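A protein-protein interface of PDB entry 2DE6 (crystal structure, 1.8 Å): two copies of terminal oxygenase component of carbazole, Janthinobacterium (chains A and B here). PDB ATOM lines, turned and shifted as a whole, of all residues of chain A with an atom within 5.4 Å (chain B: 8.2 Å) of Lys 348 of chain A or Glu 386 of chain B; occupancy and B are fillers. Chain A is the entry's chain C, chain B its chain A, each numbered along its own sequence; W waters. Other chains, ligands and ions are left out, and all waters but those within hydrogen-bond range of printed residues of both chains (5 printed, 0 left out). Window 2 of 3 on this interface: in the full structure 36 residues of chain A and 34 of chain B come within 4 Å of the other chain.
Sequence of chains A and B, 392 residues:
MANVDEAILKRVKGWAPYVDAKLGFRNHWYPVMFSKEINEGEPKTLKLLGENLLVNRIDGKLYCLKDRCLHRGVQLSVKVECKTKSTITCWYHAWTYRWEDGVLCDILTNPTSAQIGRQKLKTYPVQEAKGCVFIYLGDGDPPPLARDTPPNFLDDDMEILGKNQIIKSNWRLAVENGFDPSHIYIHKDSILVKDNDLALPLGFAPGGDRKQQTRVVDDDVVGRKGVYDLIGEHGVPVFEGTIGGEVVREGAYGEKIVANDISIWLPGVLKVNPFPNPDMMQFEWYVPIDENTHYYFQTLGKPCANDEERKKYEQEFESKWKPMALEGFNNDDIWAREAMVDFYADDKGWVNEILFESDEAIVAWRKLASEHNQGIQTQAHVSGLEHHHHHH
No position is printed for both chains. Of the 4 pairs that touch across the chains among the printed residues, none has its exchanged pair printed and touching as well.
Phe 343 of chain A touches Arg 68 of chain B. Asp 346 of chain A touches Ser 383 of chain B.
O of Ser 383 of chain B is in hydrogen-bond range of ND2 of Asn 352 of chain A (3.4 Å). The side-chain carboxylate (OE1) of Glu 386 of chain B is in salt-bridge range of the side-chain amino group (NZ) of Lys 348 of chain A, at 3.5 Å.
Water W5 bridges the side-chain amide oxygen of Asn 352 of chain A and the backbone carbonyl oxygen of Leu 385 of chain B. Water W3 lies within hydrogen-bond range of the backbone carbonyl oxygen of Gly 384 of chain B (2.6 Å), the side-chain hydroxyl of Ser 383 of chain B (2.8 Å), the side-chain carboxylate of Glu 386 of chain B (2.9 Å) and the side-chain amide nitrogen of Asn 352 of chain A (3.2 Å). Water W4 bridges ND2 of Asn 352 of chain A (2.7 Å) and O of Ser 383 of chain B (2.9 Å). Water W2 bridges OD2 of Asp 346 of chain A (2.8 Å) and NE2 of Gln 379 of chain B (3.2 Å). Water W1 lies within hydrogen-bond range of the side-chain hydroxyl (OG) of Ser 383 of chain B (2.8 Å) and the side-chain amino group (NZ) of Lys 348 of chain A (2.8 Å).
Lys 348 of chain A touches just one residue of chain B: Glu 386 (3.5 Å). No residue of chain B comes within 4 Å of Gly 349 of chain A. Printed residues of chain B within 4 Å of Phe 343 of chain A: Arg 68. Printed residues of chain B within 4 Å of Asp 346 of chain A: Ser 383. Of the printed residues of chain A, Ser 383 of chain B touches Asp 346 (3.8 Å) and Asn 352 (3.4 Å). Printed residues of chain A within 4 Å of Arg 68 of chain B: Phe 343 (3.9 Å). Ile 8 of chain A touches none of the printed residues of chain B. His 389 of chain B touches none of the printed residues of chain A. The nearest printed residue of chain A that does not touch Glu 386 of chain B is Asn 352 of chain A (5.6 Å). The nearest printed residue of chain A that does not touch Ser 383 of chain B is Lys 348 of chain A (4.3 Å).
The guanidinium group of Arg 68 of chain B lies within hydrogen-bond range of the backbone carbonyl oxygen of Val 382 of chain B (2.7 Å). The backbone carbonyl oxygen of Gln 379 of chain B sits at hydrogen-bond distance from the side-chain hydroxyl of Ser 383 of chain B, 3.4 Å away. O of Phe 343 of chain A lies within hydrogen-bond range of N of Gly 349 of chain A. The side-chain carboxylate (OD1) of Asp 346 of chain A sits at hydrogen-bond distance from the backbone NH (N) of Lys 348 of chain A, at 2.9 Å. The side-chain amide nitrogen of Asn 352 of chain A lies within hydrogen-bond range of the backbone carbonyl oxygen of Lys 348 of chain A, 3.3 Å away.
Of the 11 printed residues of chain A, 4 touch a printed residue of chain B. Of the 13 printed residues of chain B, 3 touch a printed residue of chain A.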
ATOM      1  N   ILE A   8      -5.002  -7.343  29.843  1.00  0.00           N
ATOM      2  CA  ILE A   8      -6.398  -7.761  29.886  1.00  0.00           C
ATOM      3  C   ILE A   8      -7.315  -6.571  30.177  1.00  0.00           C
ATOM      4  O   ILE A   8      -8.361  -6.411  29.546  1.00  0.00           O
ATOM      5  CB  ILE A   8      -6.607  -8.865  30.954  1.00  0.00           C
ATOM      6  CG1 ILE A   8      -5.880 -10.140  30.523  1.00  0.00           C
ATOM      7  CG2 ILE A   8      -8.093  -9.141  31.150  1.00  0.00           C
ATOM      8  CD1 ILE A   8      -5.998 -11.289  31.514  1.00  0.00           C
ATOM      9  N   PHE A 343     -13.027 -21.047  33.924  1.00  0.00           N
ATOM     10  CA  PHE A 343     -12.961 -20.153  32.772  1.00  0.00           C
ATOM     11  C   PHE A 343     -12.450 -18.758  33.124  1.00  0.00           C
ATOM     12  O   PHE A 343     -11.712 -18.152  32.349  1.00  0.00           O
ATOM     13  CB  PHE A 343     -14.348 -20.058  32.129  1.00  0.00           C
ATOM     14  CG  PHE A 343     -14.358 -19.399  30.780  1.00  0.00           C
ATOM     15  CD1 PHE A 343     -13.557 -19.881  29.746  1.00  0.00           C
ATOM     16  CD2 PHE A 343     -15.223 -18.339  30.521  1.00  0.00           C
ATOM     17  CE1 PHE A 343     -13.626 -19.318  28.472  1.00  0.00           C
ATOM     18  CE2 PHE A 343     -15.297 -17.769  29.247  1.00  0.00           C
ATOM     19  CZ  PHE A 343     -14.497 -18.263  28.223  1.00  0.00           C
ATOM     20  N   TYR A 344     -12.835 -18.261  34.296  1.00  0.00           N
ATOM     21  CA  TYR A 344     -12.441 -16.925  34.733  1.00  0.00           C
ATOM     22  C   TYR A 344     -11.249 -16.868  35.685  1.00  0.00           C
ATOM     23  O   TYR A 344     -10.731 -15.787  35.954  1.00  0.00           O
ATOM     24  CB  TYR A 344     -13.640 -16.230  35.389  1.00  0.00           C
ATOM     25  CG  TYR A 344     -14.727 -15.880  34.405  1.00  0.00           C
ATOM     26  CD1 TYR A 344     -14.678 -14.689  33.679  1.00  0.00           C
ATOM     27  CD2 TYR A 344     -15.769 -16.767  34.146  1.00  0.00           C
ATOM     28  CE1 TYR A 344     -15.639 -14.394  32.715  1.00  0.00           C
ATOM     29  CE2 TYR A 344     -16.734 -16.480  33.181  1.00  0.00           C
ATOM     30  CZ  TYR A 344     -16.663 -15.296  32.471  1.00  0.00           C
ATOM     31  OH  TYR A 344     -17.607 -15.017  31.503  1.00  0.00           O
ATOM     32  N   ASP A 346      -8.104 -17.556  35.363  1.00  0.00           N
ATOM     33  CA  ASP A 346      -6.872 -16.995  34.819  1.00  0.00           C
ATOM     34  C   ASP A 346      -7.139 -15.598  34.267  1.00  0.00           C
ATOM     35  O   ASP A 346      -6.288 -15.008  33.600  1.00  0.00           O
ATOM     36  CB  ASP A 346      -6.326 -17.900  33.709  1.00  0.00           C
ATOM     37  CG  ASP A 346      -7.379 -18.252  32.671  1.00  0.00           C
ATOM     38  OD1 ASP A 346      -8.472 -17.654  32.708  1.00  0.00           O
ATOM     39  OD2 ASP A 346      -7.112 -19.128  31.815  1.00  0.00           O
ATOM     40  N   ASP A 347      -8.331 -15.085  34.566  1.00  0.00           N
ATOM     41  CA  ASP A 347      -8.785 -13.772  34.118  1.00  0.00           C
ATOM     42  C   ASP A 347      -9.043 -13.725  32.610  1.00  0.00           C
ATOM     43  O   ASP A 347      -9.409 -12.678  32.074  1.00  0.00           O
ATOM     44  CB  ASP A 347      -7.773 -12.678  34.496  1.00  0.00           C
ATOM     45  CG  ASP A 347      -7.690 -12.444  35.999  1.00  0.00           C
ATOM     46  OD1 ASP A 347      -8.751 -12.384  36.655  1.00  0.00           O
ATOM     47  OD2 ASP A 347      -6.563 -12.303  36.525  1.00  0.00           O
ATOM     48  N   LYS A 348      -8.871 -14.857  31.932  1.00  0.00           N
ATOM     49  CA  LYS A 348      -9.065 -14.906  30.482  1.00  0.00           C
ATOM     50  C   LYS A 348     -10.531 -14.978  30.050  1.00  0.00           C
ATOM     51  O   LYS A 348     -10.877 -14.567  28.940  1.00  0.00           O
ATOM     52  CB  LYS A 348      -8.285 -16.083  29.885  1.00  0.00           C
ATOM     53  CG  LYS A 348      -6.776 -16.039  30.149  1.00  0.00           C
ATOM     54  CD  LYS A 348      -6.154 -14.742  29.648  1.00  0.00           C
ATOM     55  CE  LYS A 348      -4.649 -14.689  29.905  1.00  0.00           C
ATOM     56  NZ  LYS A 348      -3.880 -15.687  29.112  1.00  0.00           N
ATOM     57  N   GLY A 349     -11.388 -15.503  30.922  1.00  0.00           N
ATOM     58  CA  GLY A 349     -12.799 -15.590  30.589  1.00  0.00           C
ATOM     59  C   GLY A 349     -13.406 -14.220  30.339  1.00  0.00           C
ATOM     60  O   GLY A 349     -14.375 -14.086  29.586  1.00  0.00           O
ATOM     61  N   TRP A 350     -12.839 -13.193  30.971  1.00  0.00           N
ATOM     62  CA  TRP A 350     -13.332 -11.828  30.804  1.00  0.00           C
ATOM     63  C   TRP A 350     -13.087 -11.324  29.385  1.00  0.00           C
ATOM     64  O   TRP A 350     -13.613 -10.284  28.983  1.00  0.00           O
ATOM     65  CB  TRP A 350     -12.662 -10.884  31.808  1.00  0.00           C
ATOM     66  CG  TRP A 350     -12.929 -11.241  33.237  1.00  0.00           C
ATOM     67  CD1 TRP A 350     -12.031 -11.738  34.140  1.00  0.00           C
ATOM     68  CD2 TRP A 350     -14.185 -11.161  33.922  1.00  0.00           C
ATOM     69  NE1 TRP A 350     -12.651 -11.977  35.344  1.00  0.00           N
ATOM     70  CE2 TRP A 350     -13.974 -11.631  35.239  1.00  0.00           C
ATOM     71  CE3 TRP A 350     -15.471 -10.740  33.551  1.00  0.00           C
ATOM     72  CZ2 TRP A 350     -15.002 -11.693  36.187  1.00  0.00           C
ATOM     73  CZ3 TRP A 350     -16.497 -10.802  34.497  1.00  0.00           C
ATOM     74  CH2 TRP A 350     -16.253 -11.275  35.799  1.00  0.00           C
ATOM     75  N   VAL A 351     -12.278 -12.060  28.633  1.00  0.00           N
ATOM     76  CA  VAL A 351     -11.986 -11.698  27.252  1.00  0.00           C
ATOM     77  C   VAL A 351     -12.602 -12.689  26.261  1.00  0.00           C
ATOM     78  O   VAL A 351     -13.115 -12.288  25.217  1.00  0.00           O
ATOM     79  CB  VAL A 351     -10.458 -11.658  26.984  1.00  0.00           C
ATOM     80  CG1 VAL A 351     -10.196 -11.428  25.495  1.00  0.00           C
ATOM     81  CG2 VAL A 351      -9.805 -10.556  27.803  1.00  0.00           C
ATOM     82  N   ASN A 352     -12.580 -13.975  26.606  1.00  0.00           N
ATOM     83  CA  ASN A 352     -13.064 -15.017  25.703  1.00  0.00           C
ATOM     84  C   ASN A 352     -14.545 -15.402  25.716  1.00  0.00           C
ATOM     85  O   ASN A 352     -15.003 -16.111  24.821  1.00  0.00           O
ATOM     86  CB  ASN A 352     -12.205 -16.266  25.888  1.00  0.00           C
ATOM     87  CG  ASN A 352     -10.751 -16.018  25.526  1.00  0.00           C
ATOM     88  OD1 ASN A 352     -10.458 -15.462  24.471  1.00  0.00           O
ATOM     89  ND2 ASN A 352      -9.838 -16.434  26.395  1.00  0.00           N
ATOM     90  N   GLU A 353     -15.283 -14.940  26.718  1.00  0.00           N
ATOM     91  CA  GLU A 353     -16.712 -15.232  26.821  1.00  0.00           C
ATOM     92  C   GLU A 353     -17.446 -14.806  25.548  1.00  0.00           C
ATOM     93  O   GLU A 353     -17.150 -13.755  24.985  1.00  0.00           O
ATOM     94  CB  GLU A 353     -17.308 -14.466  28.008  1.00  0.00           C
ATOM     95  CG  GLU A 353     -16.996 -12.964  27.941  1.00  0.00           C
ATOM     96  CD  GLU A 353     -17.551 -12.156  29.102  1.00  0.00           C
ATOM     97  OE1 GLU A 353     -17.823 -12.730  30.179  1.00  0.00           O
ATOM     98  OE2 GLU A 353     -17.693 -10.924  28.935  1.00  0.00           O
ATOM     99  N   ARG B  68     -16.423 -27.421  26.898  1.00  0.00           N
ATOM    100  CA  ARG B  68     -16.426 -26.051  27.402  1.00  0.00           C
ATOM    101  C   ARG B  68     -17.400 -25.238  26.571  1.00  0.00           C
ATOM    102  O   ARG B  68     -17.179 -25.015  25.382  1.00  0.00           O
ATOM    103  CB  ARG B  68     -15.044 -25.402  27.317  1.00  0.00           C
ATOM    104  CG  ARG B  68     -15.034 -24.015  27.966  1.00  0.00           C
ATOM    105  CD  ARG B  68     -13.660 -23.381  27.945  1.00  0.00           C
ATOM    106  NE  ARG B  68     -13.237 -23.074  26.589  1.00  0.00           N
ATOM    107  CZ  ARG B  68     -11.980 -22.831  26.242  1.00  0.00           C
ATOM    108  NH1 ARG B  68     -11.022 -22.860  27.160  1.00  0.00           N
ATOM    109  NH2 ARG B  68     -11.681 -22.568  24.980  1.00  0.00           N
ATOM    110  N   THR B 378       0.289 -24.901  23.525  1.00  0.00           N
ATOM    111  CA  THR B 378       0.563 -23.825  24.477  1.00  0.00           C
ATOM    112  C   THR B 378      -0.641 -23.613  25.388  1.00  0.00           C
ATOM    113  O   THR B 378      -1.745 -24.068  25.086  1.00  0.00           O
ATOM    114  CB  THR B 378       0.861 -22.493  23.757  1.00  0.00           C
ATOM    115  OG1 THR B 378      -0.331 -22.004  23.130  1.00  0.00           O
ATOM    116  CG2 THR B 378       1.909 -22.690  22.687  1.00  0.00           C
ATOM    117  N   GLN B 379      -0.437 -22.917  26.501  1.00  0.00           N
ATOM    118  CA  GLN B 379      -1.538 -22.668  27.424  1.00  0.00           C
ATOM    119  C   GLN B 379      -2.603 -21.824  26.725  1.00  0.00           C
ATOM    120  O   GLN B 379      -3.784 -21.891  27.071  1.00  0.00           O
ATOM    121  CB  GLN B 379      -1.027 -21.953  28.681  1.00  0.00           C
ATOM    122  CG  GLN B 379      -2.062 -21.795  29.786  1.00  0.00           C
ATOM    123  CD  GLN B 379      -2.722 -23.107  30.176  1.00  0.00           C
ATOM    124  OE1 GLN B 379      -2.077 -24.155  30.219  1.00  0.00           O
ATOM    125  NE2 GLN B 379      -4.018 -23.049  30.479  1.00  0.00           N
ATOM    126  N   ALA B 380      -2.182 -21.037  25.736  1.00  0.00           N
ATOM    127  CA  ALA B 380      -3.116 -20.196  24.990  1.00  0.00           C
ATOM    128  C   ALA B 380      -4.067 -21.059  24.165  1.00  0.00           C
ATOM    129  O   ALA B 380      -5.202 -20.661  23.910  1.00  0.00           O
ATOM    130  CB  ALA B 380      -2.358 -19.230  24.081  1.00  0.00           C
ATOM    131  N   HIS B 381      -3.604 -22.231  23.731  1.00  0.00           N
ATOM    132  CA  HIS B 381      -4.470 -23.133  22.971  1.00  0.00           C
ATOM    133  C   HIS B 381      -5.579 -23.595  23.910  1.00  0.00           C
ATOM    134  O   HIS B 381      -6.725 -23.778  23.503  1.00  0.00           O
ATOM    135  CB  HIS B 381      -3.709 -24.372  22.470  1.00  0.00           C
ATOM    136  CG  HIS B 381      -2.892 -24.135  21.236  1.00  0.00           C
ATOM    137  ND1 HIS B 381      -1.541 -23.860  21.276  1.00  0.00           N
ATOM    138  CD2 HIS B 381      -3.235 -24.143  19.926  1.00  0.00           C
ATOM    139  CE1 HIS B 381      -1.087 -23.711  20.043  1.00  0.00           C
ATOM    140  NE2 HIS B 381      -2.095 -23.878  19.206  1.00  0.00           N
ATOM    141  N   VAL B 382      -5.221 -23.791  25.175  1.00  0.00           N
ATOM    142  CA  VAL B 382      -6.180 -24.242  26.171  1.00  0.00           C
ATOM    143  C   VAL B 382      -7.215 -23.181  26.531  1.00  0.00           C
ATOM    144  O   VAL B 382      -8.409 -23.479  26.590  1.00  0.00           O
ATOM    145  CB  VAL B 382      -5.469 -24.701  27.472  1.00  0.00           C
ATOM    146  CG1 VAL B 382      -6.501 -25.116  28.511  1.00  0.00           C
ATOM    147  CG2 VAL B 382      -4.534 -25.864  27.169  1.00  0.00           C
ATOM    148  N   SER B 383      -6.772 -21.948  26.776  1.00  0.00           N
ATOM    149  CA  SER B 383      -7.708 -20.882  27.147  1.00  0.00           C
ATOM    150  C   SER B 383      -8.331 -20.178  25.944  1.00  0.00           C
ATOM    151  O   SER B 383      -9.495 -19.774  25.983  1.00  0.00           O
ATOM    152  CB  SER B 383      -7.014 -19.844  28.043  1.00  0.00           C
ATOM    153  OG  SER B 383      -5.930 -19.232  27.372  1.00  0.00           O
ATOM    154  N   GLY B 384      -7.553 -20.039  24.877  1.00  0.00           N
ATOM    155  CA  GLY B 384      -8.032 -19.377  23.675  1.00  0.00           C
ATOM    156  C   GLY B 384      -6.878 -18.619  23.049  1.00  0.00           C
ATOM    157  O   GLY B 384      -6.318 -17.717  23.673  1.00  0.00           O
ATOM    158  N   LEU B 385      -6.512 -18.986  21.826  1.00  0.00           N
ATOM    159  CA  LEU B 385      -5.391 -18.341  21.152  1.00  0.00           C
ATOM    160  C   LEU B 385      -5.522 -16.831  21.157  1.00  0.00           C
ATOM    161  O   LEU B 385      -6.614 -16.286  21.006  1.00  0.00           O
ATOM    162  CB  LEU B 385      -5.260 -18.857  19.718  1.00  0.00           C
ATOM    163  CG  LEU B 385      -4.754 -20.300  19.591  1.00  0.00           C
ATOM    164  CD1 LEU B 385      -4.764 -20.715  18.128  1.00  0.00           C
ATOM    165  CD2 LEU B 385      -3.344 -20.409  20.178  1.00  0.00           C
ATOM    166  N   GLU B 386      -4.397 -16.151  21.341  1.00  0.00           N
ATOM    167  CA  GLU B 386      -4.419 -14.701  21.381  1.00  0.00           C
ATOM    168  C   GLU B 386      -3.452 -14.031  20.424  1.00  0.00           C
ATOM    169  O   GLU B 386      -2.343 -14.512  20.184  1.00  0.00           O
ATOM    170  CB  GLU B 386      -4.179 -14.212  22.814  1.00  0.00           C
ATOM    171  CG  GLU B 386      -3.375 -15.158  23.682  1.00  0.00           C
ATOM    172  CD  GLU B 386      -3.436 -14.796  25.159  1.00  0.00           C
ATOM    173  OE1 GLU B 386      -4.518 -14.935  25.778  1.00  0.00           O
ATOM    174  OE2 GLU B 386      -2.397 -14.369  25.700  1.00  0.00           O
ATOM    175  N   HIS B 387      -3.909 -12.915  19.871  1.00  0.00           N
ATOM    176  CA  HIS B 387      -3.133 -12.112  18.937  1.00  0.00           C
ATOM    177  C   HIS B 387      -3.672 -10.692  19.015  1.00  0.00           C
ATOM    178  O   HIS B 387      -4.880 -10.474  18.911  1.00  0.00           O
ATOM    179  CB  HIS B 387      -3.286 -12.634  17.512  1.00  0.00           C
ATOM    180  CG  HIS B 387      -2.545 -11.821  16.499  1.00  0.00           C
ATOM    181  ND1 HIS B 387      -1.169 -11.798  16.428  1.00  0.00           N
ATOM    182  CD2 HIS B 387      -2.986 -10.962  15.549  1.00  0.00           C
ATOM    183  CE1 HIS B 387      -0.792 -10.961  15.478  1.00  0.00           C
ATOM    184  NE2 HIS B 387      -1.875 -10.440  14.929  1.00  0.00           N
ATOM    185  N   HIS B 388      -2.777  -9.728  19.210  1.00  0.00           N
ATOM    186  CA  HIS B 388      -3.172  -8.328  19.311  1.00  0.00           C
ATOM    187  C   HIS B 388      -2.547  -7.567  18.143  1.00  0.00           C
ATOM    188  O   HIS B 388      -1.328  -7.394  18.086  1.00  0.00           O
ATOM    189  CB  HIS B 388      -2.696  -7.761  20.653  1.00  0.00           C
ATOM    190  CG  HIS B 388      -3.440  -6.539  21.099  1.00  0.00           C
ATOM    191  ND1 HIS B 388      -3.344  -5.328  20.449  1.00  0.00           N
ATOM    192  CD2 HIS B 388      -4.287  -6.343  22.137  1.00  0.00           C
ATOM    193  CE1 HIS B 388      -4.101  -4.438  21.068  1.00  0.00           C
ATOM    194  NE2 HIS B 388      -4.684  -5.028  22.095  1.00  0.00           N
ATOM    195  N   HIS B 389      -3.389  -7.130  17.209  1.00  0.00           N
ATOM    196  CA  HIS B 389      -2.939  -6.405  16.021  1.00  0.00           C
ATOM    197  C   HIS B 389      -2.068  -5.196  16.367  1.00  0.00           C
ATOM    198  O   HIS B 389      -1.072  -4.976  15.646  1.00  0.00           O
ATOM    199  CB  HIS B 389      -4.149  -5.962  15.183  1.00  0.00           C
ATOM    200  CG  HIS B 389      -4.630  -4.577  15.490  1.00  0.00           C
ATOM    201  ND1 HIS B 389      -4.037  -3.451  14.961  1.00  0.00           N
ATOM    202  CD2 HIS B 389      -5.625  -4.136  16.295  1.00  0.00           C
ATOM    203  CE1 HIS B 389      -4.645  -2.375  15.426  1.00  0.00           C
ATOM    204  NE2 HIS B 389      -5.613  -2.762  16.239  1.00  0.00           N
HETATM  205  O   HOH W   1      -3.677 -18.505  28.781  1.00  0.00           O
HETATM  206  O   HOH W   2      -4.600 -19.985  31.087  1.00  0.00           O
HETATM  207  O   HOH W   3      -6.707 -16.831  26.118  1.00  0.00           O
HETATM  208  O   HOH W   4     -10.461 -18.327  28.284  1.00  0.00           O
HETATM  209  O   HOH W   5      -8.378 -14.862  22.993  1.00  0.00           O
